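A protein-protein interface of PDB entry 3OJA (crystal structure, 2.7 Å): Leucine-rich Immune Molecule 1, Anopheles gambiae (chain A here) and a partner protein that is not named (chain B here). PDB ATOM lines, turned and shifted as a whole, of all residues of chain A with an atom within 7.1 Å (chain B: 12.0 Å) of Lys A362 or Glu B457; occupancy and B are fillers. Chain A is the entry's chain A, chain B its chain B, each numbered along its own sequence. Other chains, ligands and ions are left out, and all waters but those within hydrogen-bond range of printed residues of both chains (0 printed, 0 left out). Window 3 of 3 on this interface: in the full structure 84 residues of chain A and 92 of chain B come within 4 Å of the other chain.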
ATOM      1  N   VAL A  69      23.594 -24.871  30.652  1.00  0.00           N
ATOM      2  CA  VAL A  69      23.901 -24.459  29.288  1.00  0.00           C
ATOM      3  C   VAL A  69      25.140 -25.166  28.834  1.00  0.00           C
ATOM      4  O   VAL A  69      26.048 -24.512  28.374  1.00  0.00           O
ATOM      5  CB  VAL A  69      24.119 -22.934  29.132  1.00  0.00           C
ATOM      6  CG1 VAL A  69      22.841 -22.209  29.299  1.00  0.00           C
ATOM      7  CG2 VAL A  69      25.131 -22.447  30.110  1.00  0.00           C
ATOM      8  N   THR A 356      19.782 -16.836  37.630  1.00  0.00           N
ATOM      9  CA  THR A 356      20.582 -17.810  36.893  1.00  0.00           C
ATOM     10  C   THR A 356      20.095 -17.845  35.452  1.00  0.00           C
ATOM     11  O   THR A 356      20.829 -18.326  34.597  1.00  0.00           O
ATOM     12  CB  THR A 356      20.605 -19.264  37.487  1.00  0.00           C
ATOM     13  OG1 THR A 356      19.344 -19.878  37.261  1.00  0.00           O
ATOM     14  CG2 THR A 356      20.980 -19.311  39.003  1.00  0.00           C
ATOM     15  N   LEU A 357      18.873 -17.362  35.177  1.00  0.00           N
ATOM     16  CA  LEU A 357      18.418 -17.280  33.785  1.00  0.00           C
ATOM     17  C   LEU A 357      19.326 -16.326  33.047  1.00  0.00           C
ATOM     18  O   LEU A 357      19.711 -16.603  31.914  1.00  0.00           O
ATOM     19  CB  LEU A 357      16.987 -16.800  33.619  1.00  0.00           C
ATOM     20  CG  LEU A 357      15.955 -17.878  33.897  1.00  0.00           C
ATOM     21  CD1 LEU A 357      14.587 -17.331  33.659  1.00  0.00           C
ATOM     22  CD2 LEU A 357      16.126 -19.119  33.085  1.00  0.00           C
ATOM     23  N   ARG A 358      19.690 -15.225  33.705  1.00  0.00           N
ATOM     24  CA  ARG A 358      20.492 -14.187  33.076  1.00  0.00           C
ATOM     25  C   ARG A 358      21.900 -14.665  33.019  1.00  0.00           C
ATOM     26  O   ARG A 358      22.551 -14.503  32.006  1.00  0.00           O
ATOM     27  CB  ARG A 358      20.358 -12.848  33.790  1.00  0.00           C
ATOM     28  CG  ARG A 358      18.901 -12.363  33.812  1.00  0.00           C
ATOM     29  CD  ARG A 358      18.812 -10.847  33.839  1.00  0.00           C
ATOM     30  NE  ARG A 358      17.707 -10.375  34.678  1.00  0.00           N
ATOM     31  CZ  ARG A 358      17.786 -10.175  36.004  1.00  0.00           C
ATOM     32  NH1 ARG A 358      18.930 -10.408  36.667  1.00  0.00           N
ATOM     33  NH2 ARG A 358      16.707  -9.746  36.678  1.00  0.00           N
ATOM     34  N   LYS A 359      22.358 -15.312  34.077  1.00  0.00           N
ATOM     35  CA  LYS A 359      23.659 -15.954  34.024  1.00  0.00           C
ATOM     36  C   LYS A 359      23.720 -16.940  32.839  1.00  0.00           C
ATOM     37  O   LYS A 359      24.753 -17.030  32.174  1.00  0.00           O
ATOM     38  CB  LYS A 359      24.002 -16.646  35.356  1.00  0.00           C
ATOM     39  CG  LYS A 359      24.461 -15.699  36.512  1.00  0.00           C
ATOM     40  CD  LYS A 359      25.096 -16.454  37.682  1.00  0.00           C
ATOM     41  CE  LYS A 359      26.150 -15.636  38.415  1.00  0.00           C
ATOM     42  NZ  LYS A 359      27.560 -15.838  37.870  1.00  0.00           N
ATOM     43  N   GLN A 360      22.620 -17.659  32.569  1.00  0.00           N
ATOM     44  CA  GLN A 360      22.548 -18.643  31.460  1.00  0.00           C
ATOM     45  C   GLN A 360      22.510 -17.938  30.090  1.00  0.00           C
ATOM     46  O   GLN A 360      23.198 -18.366  29.154  1.00  0.00           O
ATOM     47  CB  GLN A 360      21.304 -19.552  31.551  1.00  0.00           C
ATOM     48  CG  GLN A 360      21.464 -20.828  32.369  1.00  0.00           C
ATOM     49  CD  GLN A 360      20.150 -21.636  32.472  1.00  0.00           C
ATOM     50  OE1 GLN A 360      19.090 -21.168  32.074  1.00  0.00           O
ATOM     51  NE2 GLN A 360      20.231 -22.839  32.996  1.00  0.00           N
ATOM     52  N   ALA A 361      21.695 -16.874  29.989  1.00  0.00           N
ATOM     53  CA  ALA A 361      21.456 -16.153  28.736  1.00  0.00           C
ATOM     54  C   ALA A 361      22.699 -15.443  28.343  1.00  0.00           C
ATOM     55  O   ALA A 361      22.866 -15.133  27.197  1.00  0.00           O
ATOM     56  CB  ALA A 361      20.352 -15.161  28.886  1.00  0.00           C
ATOM     57  N   LYS A 362      23.600 -15.183  29.277  1.00  0.00           N
ATOM     58  CA  LYS A 362      24.862 -14.595  28.880  1.00  0.00           C
ATOM     59  C   LYS A 362      25.693 -15.576  28.076  1.00  0.00           C
ATOM     60  O   LYS A 362      26.276 -15.176  27.095  1.00  0.00           O
ATOM     61  CB  LYS A 362      25.666 -14.091  30.062  1.00  0.00           C
ATOM     62  CG  LYS A 362      27.044 -13.682  29.657  1.00  0.00           C
ATOM     63  CD  LYS A 362      27.674 -12.790  30.673  1.00  0.00           C
ATOM     64  CE  LYS A 362      29.183 -12.813  30.554  1.00  0.00           C
ATOM     65  NZ  LYS A 362      29.829 -12.614  31.911  1.00  0.00           N
ATOM     66  N   ILE A 363      25.778 -16.836  28.486  1.00  0.00           N
ATOM     67  CA  ILE A 363      26.629 -17.797  27.792  1.00  0.00           C
ATOM     68  C   ILE A 363      26.004 -18.210  26.449  1.00  0.00           C
ATOM     69  O   ILE A 363      26.678 -18.475  25.457  1.00  0.00           O
ATOM     70  CB  ILE A 363      26.832 -19.040  28.645  1.00  0.00           C
ATOM     71  CG1 ILE A 363      27.696 -18.683  29.851  1.00  0.00           C
ATOM     72  CG2 ILE A 363      27.460 -20.140  27.875  1.00  0.00           C
ATOM     73  CD1 ILE A 363      27.831 -19.802  30.875  1.00  0.00           C
ATOM     74  N   THR A 364      24.689 -18.275  26.442  1.00  0.00           N
ATOM     75  CA  THR A 364      23.944 -18.688  25.293  1.00  0.00           C
ATOM     76  C   THR A 364      24.055 -17.607  24.213  1.00  0.00           C
ATOM     77  O   THR A 364      24.176 -17.931  23.040  1.00  0.00           O
ATOM     78  CB  THR A 364      22.473 -18.937  25.716  1.00  0.00           C
ATOM     79  OG1 THR A 364      22.317 -20.311  26.033  1.00  0.00           O
ATOM     80  CG2 THR A 364      21.482 -18.583  24.608  1.00  0.00           C
ATOM     81  N   LEU A 365      23.991 -16.331  24.618  1.00  0.00           N
ATOM     82  CA  LEU A 365      24.133 -15.205  23.700  1.00  0.00           C
ATOM     83  C   LEU A 365      25.578 -15.105  23.174  1.00  0.00           C
ATOM     84  O   LEU A 365      25.787 -14.853  22.020  1.00  0.00           O
ATOM     85  CB  LEU A 365      23.664 -13.906  24.341  1.00  0.00           C
ATOM     86  CG  LEU A 365      22.138 -13.843  24.506  1.00  0.00           C
ATOM     87  CD1 LEU A 365      21.692 -12.521  25.101  1.00  0.00           C
ATOM     88  CD2 LEU A 365      21.407 -14.085  23.195  1.00  0.00           C
ATOM     89  N   GLU A 366      26.572 -15.354  24.001  1.00  0.00           N
ATOM     90  CA  GLU A 366      27.896 -15.500  23.479  1.00  0.00           C
ATOM     91  C   GLU A 366      27.997 -16.585  22.432  1.00  0.00           C
ATOM     92  O   GLU A 366      28.746 -16.421  21.513  1.00  0.00           O
ATOM     93  CB  GLU A 366      28.904 -15.778  24.568  1.00  0.00           C
ATOM     94  CG  GLU A 366      29.642 -14.553  24.971  1.00  0.00           C
ATOM     95  CD  GLU A 366      29.874 -14.530  26.483  1.00  0.00           C
ATOM     96  OE1 GLU A 366      30.010 -15.639  27.076  1.00  0.00           O
ATOM     97  OE2 GLU A 366      29.912 -13.411  27.081  1.00  0.00           O
ATOM     98  N   GLN A 367      27.291 -17.697  22.529  1.00  0.00           N
ATOM     99  CA  GLN A 367      27.381 -18.652  21.453  1.00  0.00           C
ATOM    100  C   GLN A 367      26.633 -18.159  20.207  1.00  0.00           C
ATOM    101  O   GLN A 367      27.138 -18.333  19.136  1.00  0.00           O
ATOM    102  CB  GLN A 367      26.946 -20.040  21.885  1.00  0.00           C
ATOM    103  CG  GLN A 367      27.732 -20.556  23.085  1.00  0.00           C
ATOM    104  CD  GLN A 367      29.249 -20.750  22.812  1.00  0.00           C
ATOM    105  OE1 GLN A 367      29.679 -21.839  22.354  1.00  0.00           O
ATOM    106  NE2 GLN A 367      30.066 -19.713  23.129  1.00  0.00           N
ATOM    107  N   LEU B 454      24.466  -5.514  37.222  1.00  0.00           N
ATOM    108  CA  LEU B 454      24.739  -5.393  35.783  1.00  0.00           C
ATOM    109  C   LEU B 454      24.456  -6.712  34.954  1.00  0.00           C
ATOM    110  O   LEU B 454      25.308  -7.606  34.783  1.00  0.00           O
ATOM    111  CB  LEU B 454      26.160  -4.813  35.552  1.00  0.00           C
ATOM    112  CG  LEU B 454      27.440  -5.686  35.592  1.00  0.00           C
ATOM    113  CD1 LEU B 454      27.725  -6.413  34.268  1.00  0.00           C
ATOM    114  CD2 LEU B 454      28.650  -4.859  35.949  1.00  0.00           C
ATOM    115  N   GLU B 455      23.207  -6.825  34.501  1.00  0.00           N
ATOM    116  CA  GLU B 455      22.840  -7.675  33.377  1.00  0.00           C
ATOM    117  C   GLU B 455      22.984  -6.775  32.136  1.00  0.00           C
ATOM    118  O   GLU B 455      22.228  -6.872  31.156  1.00  0.00           O
ATOM    119  CB  GLU B 455      21.393  -8.149  33.525  1.00  0.00           C
ATOM    120  CG  GLU B 455      20.402  -7.007  33.834  1.00  0.00           C
ATOM    121  CD  GLU B 455      18.981  -7.249  33.298  1.00  0.00           C
ATOM    122  OE1 GLU B 455      18.022  -6.661  33.865  1.00  0.00           O
ATOM    123  OE2 GLU B 455      18.828  -8.013  32.307  1.00  0.00           O
ATOM    124  N   ALA B 456      23.937  -5.852  32.208  1.00  0.00           N
ATOM    125  CA  ALA B 456      24.185  -4.937  31.109  1.00  0.00           C
ATOM    126  C   ALA B 456      24.994  -5.702  30.086  1.00  0.00           C
ATOM    127  O   ALA B 456      25.007  -5.363  28.901  1.00  0.00           O
ATOM    128  CB  ALA B 456      24.951  -3.704  31.588  1.00  0.00           C
ATOM    129  N   GLU B 457      25.687  -6.740  30.550  1.00  0.00           N
ATOM    130  CA  GLU B 457      26.417  -7.584  29.633  1.00  0.00           C
ATOM    131  C   GLU B 457      25.436  -8.387  28.786  1.00  0.00           C
ATOM    132  O   GLU B 457      25.733  -8.711  27.628  1.00  0.00           O
ATOM    133  CB  GLU B 457      27.315  -8.523  30.383  1.00  0.00           C
ATOM    134  CG  GLU B 457      28.631  -7.933  30.742  1.00  0.00           C
ATOM    135  CD  GLU B 457      29.348  -8.798  31.756  1.00  0.00           C
ATOM    136  OE1 GLU B 457      28.721  -9.777  32.229  1.00  0.00           O
ATOM    137  OE2 GLU B 457      30.517  -8.503  32.091  1.00  0.00           O
ATOM    138  N   VAL B 458      24.272  -8.703  29.358  1.00  0.00           N
ATOM    139  CA  VAL B 458      23.261  -9.456  28.629  1.00  0.00           C
ATOM    140  C   VAL B 458      22.513  -8.545  27.665  1.00  0.00           C
ATOM    141  O   VAL B 458      22.054  -8.978  26.617  1.00  0.00           O
ATOM    142  CB  VAL B 458      22.315 -10.207  29.594  1.00  0.00           C
ATOM    143  CG1 VAL B 458      20.923 -10.421  29.005  1.00  0.00           C
ATOM    144  CG2 VAL B 458      22.956 -11.523  29.966  1.00  0.00           C
ATOM    145  N   ASN B 459      22.421  -7.268  27.987  1.00  0.00           N
ATOM    146  CA  ASN B 459      21.702  -6.350  27.111  1.00  0.00           C
ATOM    147  C   ASN B 459      22.555  -5.872  25.928  1.00  0.00           C
ATOM    148  O   ASN B 459      22.015  -5.535  24.858  1.00  0.00           O
ATOM    149  CB  ASN B 459      21.181  -5.169  27.921  1.00  0.00           C
ATOM    150  CG  ASN B 459      19.991  -5.542  28.732  1.00  0.00           C
ATOM    151  OD1 ASN B 459      19.963  -5.364  29.950  1.00  0.00           O
ATOM    152  ND2 ASN B 459      18.999  -6.118  28.063  1.00  0.00           N
ATOM    153  N   GLU B 460      23.870  -5.842  26.149  1.00  0.00           N
ATOM    154  CA  GLU B 460      24.835  -5.462  25.136  1.00  0.00           C
ATOM    155  C   GLU B 460      24.906  -6.622  24.118  1.00  0.00           C
ATOM    156  O   GLU B 460      24.896  -6.418  22.898  1.00  0.00           O
ATOM    157  CB  GLU B 460      26.186  -5.158  25.806  1.00  0.00           C
ATOM    158  CG  GLU B 460      27.361  -4.959  24.860  1.00  0.00           C
ATOM    159  CD  GLU B 460      28.773  -5.057  25.540  1.00  0.00           C
ATOM    160  OE1 GLU B 460      28.885  -5.478  26.727  1.00  0.00           O
ATOM    161  OE2 GLU B 460      29.786  -4.725  24.861  1.00  0.00           O
ATOM    162  N   LEU B 461      24.913  -7.846  24.638  1.00  0.00           N
ATOM    163  CA  LEU B 461      24.857  -9.035  23.818  1.00  0.00           C
ATOM    164  C   LEU B 461      23.550  -9.161  23.048  1.00  0.00           C
ATOM    165  O   LEU B 461      23.580  -9.446  21.888  1.00  0.00           O
ATOM    166  CB  LEU B 461      25.046 -10.247  24.690  1.00  0.00           C
ATOM    167  CG  LEU B 461      26.506 -10.447  25.030  1.00  0.00           C
ATOM    168  CD1 LEU B 461      26.698 -11.367  26.225  1.00  0.00           C
ATOM    169  CD2 LEU B 461      27.183 -11.002  23.828  1.00  0.00           C
ATOM    170  N   ARG B 462      22.390  -8.967  23.643  1.00  0.00           N
ATOM    171  CA  ARG B 462      21.197  -9.060  22.822  1.00  0.00           C
ATOM    172  C   ARG B 462      21.287  -8.076  21.664  1.00  0.00           C
ATOM    173  O   ARG B 462      20.766  -8.331  20.598  1.00  0.00           O
ATOM    174  CB  ARG B 462      19.931  -8.797  23.620  1.00  0.00           C
ATOM    175  CG  ARG B 462      19.527  -9.940  24.519  1.00  0.00           C
ATOM    176  CD  ARG B 462      18.071  -9.866  24.964  1.00  0.00           C
ATOM    177  NE  ARG B 462      17.856 -10.847  26.029  1.00  0.00           N
ATOM    178  CZ  ARG B 462      17.567 -12.138  25.820  1.00  0.00           C
ATOM    179  NH1 ARG B 462      17.428 -12.584  24.572  1.00  0.00           N
ATOM    180  NH2 ARG B 462      17.399 -12.985  26.850  1.00  0.00           N
ATOM    181  N   ALA B 463      21.965  -6.956  21.878  1.00  0.00           N
ATOM    182  CA  ALA B 463      22.093  -5.919  20.857  1.00  0.00           C
ATOM    183  C   ALA B 463      23.035  -6.427  19.809  1.00  0.00           C
ATOM    184  O   ALA B 463      22.753  -6.362  18.613  1.00  0.00           O
ATOM    185  CB  ALA B 463      22.661  -4.632  21.447  1.00  0.00           C
ATOM    186  N   GLU B 464      24.178  -6.921  20.261  1.00  0.00           N
ATOM    187  CA  GLU B 464      25.169  -7.404  19.332  1.00  0.00           C
ATOM    188  C   GLU B 464      24.535  -8.469  18.407  1.00  0.00           C
ATOM    189  O   GLU B 464      24.725  -8.449  17.190  1.00  0.00           O
ATOM    190  CB  GLU B 464      26.412  -7.899  20.078  1.00  0.00           C
ATOM    191  CG  GLU B 464      27.334  -6.748  20.501  1.00  0.00           C
ATOM    192  CD  GLU B 464      28.560  -7.184  21.330  1.00  0.00           C
ATOM    193  OE1 GLU B 464      28.820  -8.416  21.454  1.00  0.00           O
ATOM    194  OE2 GLU B 464      29.265  -6.271  21.853  1.00  0.00           O
ATOM    195  N   VAL B 465      23.738  -9.350  18.979  1.00  0.00           N
ATOM    196  CA  VAL B 465      23.209 -10.464  18.249  1.00  0.00           C
ATOM    197  C   VAL B 465      22.184  -9.941  17.239  1.00  0.00           C
ATOM    198  O   VAL B 465      22.065 -10.488  16.145  1.00  0.00           O
ATOM    199  CB  VAL B 465      22.649 -11.502  19.265  1.00  0.00           C
ATOM    200  CG1 VAL B 465      21.602 -12.358  18.703  1.00  0.00           C
ATOM    201  CG2 VAL B 465      23.800 -12.343  19.810  1.00  0.00           C
ATOM    202  N   GLN B 466      21.452  -8.875  17.581  1.00  0.00           N
ATOM    203  CA  GLN B 466      20.438  -8.314  16.666  1.00  0.00           C
ATOM    204  C   GLN B 466      21.085  -7.573  15.526  1.00  0.00           C
ATOM    205  O   GLN B 466      20.587  -7.593  14.411  1.00  0.00           O
ATOM    206  CB  GLN B 466      19.461  -7.357  17.343  1.00  0.00           C
ATOM    207  CG  GLN B 466      18.132  -7.980  17.704  1.00  0.00           C
ATOM    208  CD  GLN B 466      17.250  -8.421  16.514  1.00  0.00           C
ATOM    209  OE1 GLN B 466      17.677  -8.484  15.351  1.00  0.00           O
ATOM    210  NE2 GLN B 466      15.996  -8.745  16.825  1.00  0.00           N
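NE of Arg A358 is in salt-bridge range of OE2 of Glu B455 (3.5 Å).
The side-chain carboxylate (OE1) of Glu B457 lies within salt-bridge range of the side-chain amino group (NZ) of Lys A362.
Arg A358 touches Val B458.
Val B458 touches Lys A362.
Leu B461 touches Lys A362 (CD1 to O, 3.9 Å).
Leu A365 touches Val B458.
CB of Leu B461 touches CB of Leu A365 (3.9 Å).
Leu A365 touches Arg B462 (CD1 to CG, 3.4 Å).
Leu A365 touches Val B465 (O to CG2, 3.9 Å).
OE2 of Glu A366 touches CD1 of Leu B461, at 3.9 Å.
OD1 of Asn B459 sits close to O of Glu B455 (3.0 Å).
Of the 13 printed residues of chain B, 6 touch a printed residue of chain A.
Printed residues of chain B that touch a printed residue of chain A: Glu B455, Glu B457, Val B458, Leu B461, Arg B462 and Val B465.
Hydrophobic or aromatic side chains of chain B within 4 Å of the printed part of chain A: Val B458, Leu B461 and Val B465.
Along chain A the printed residues that touch a printed residue of chain B span positions 358 to 366.
Among the printed residues, 10 pairs touch across the chains.
Of the printed residues of chain B, Arg A358 touches Glu B455 and Val B458.
Lys A359 touches none of the printed residues of chain B.
Gln A360 touches none of the printed residues of chain B.
No residue of chain B comes within 4 Å of Ala A361.
Of chain B, only Glu B457, Val B458 and Leu B461 come within 4 Å of Lys A362.
No residue of chain B comes within 4 Å of Ile A363.
No residue of chain B comes within 4 Å of Thr A364.
Of chain B, only Val B458, Leu B461, Arg B462 and Val B465 come within 4 Å of Leu A365.
Of chain B, only Leu B461 (3.9 Å) comes within 4 Å of Glu A366.
Of chain A, only Lys A362 (3.1 Å) comes within 4 Å of Glu B457.
Of the printed residues of chain A, Val B458 touches Arg A358, Lys A362 and Leu A365.
Of the printed residues of chain A, Arg B462 touches Leu A365 (3.4 Å).
The nearest residue of chain B that does not touch Lys A362 is Leu B454 (7.0 Å).
The nearest residue of chain A that does not touch Glu B457 is Leu A365 (6.1 Å).
The nearest printed residue of chain A that does not touch Arg B462 is Ala A361 (4.2 Å).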
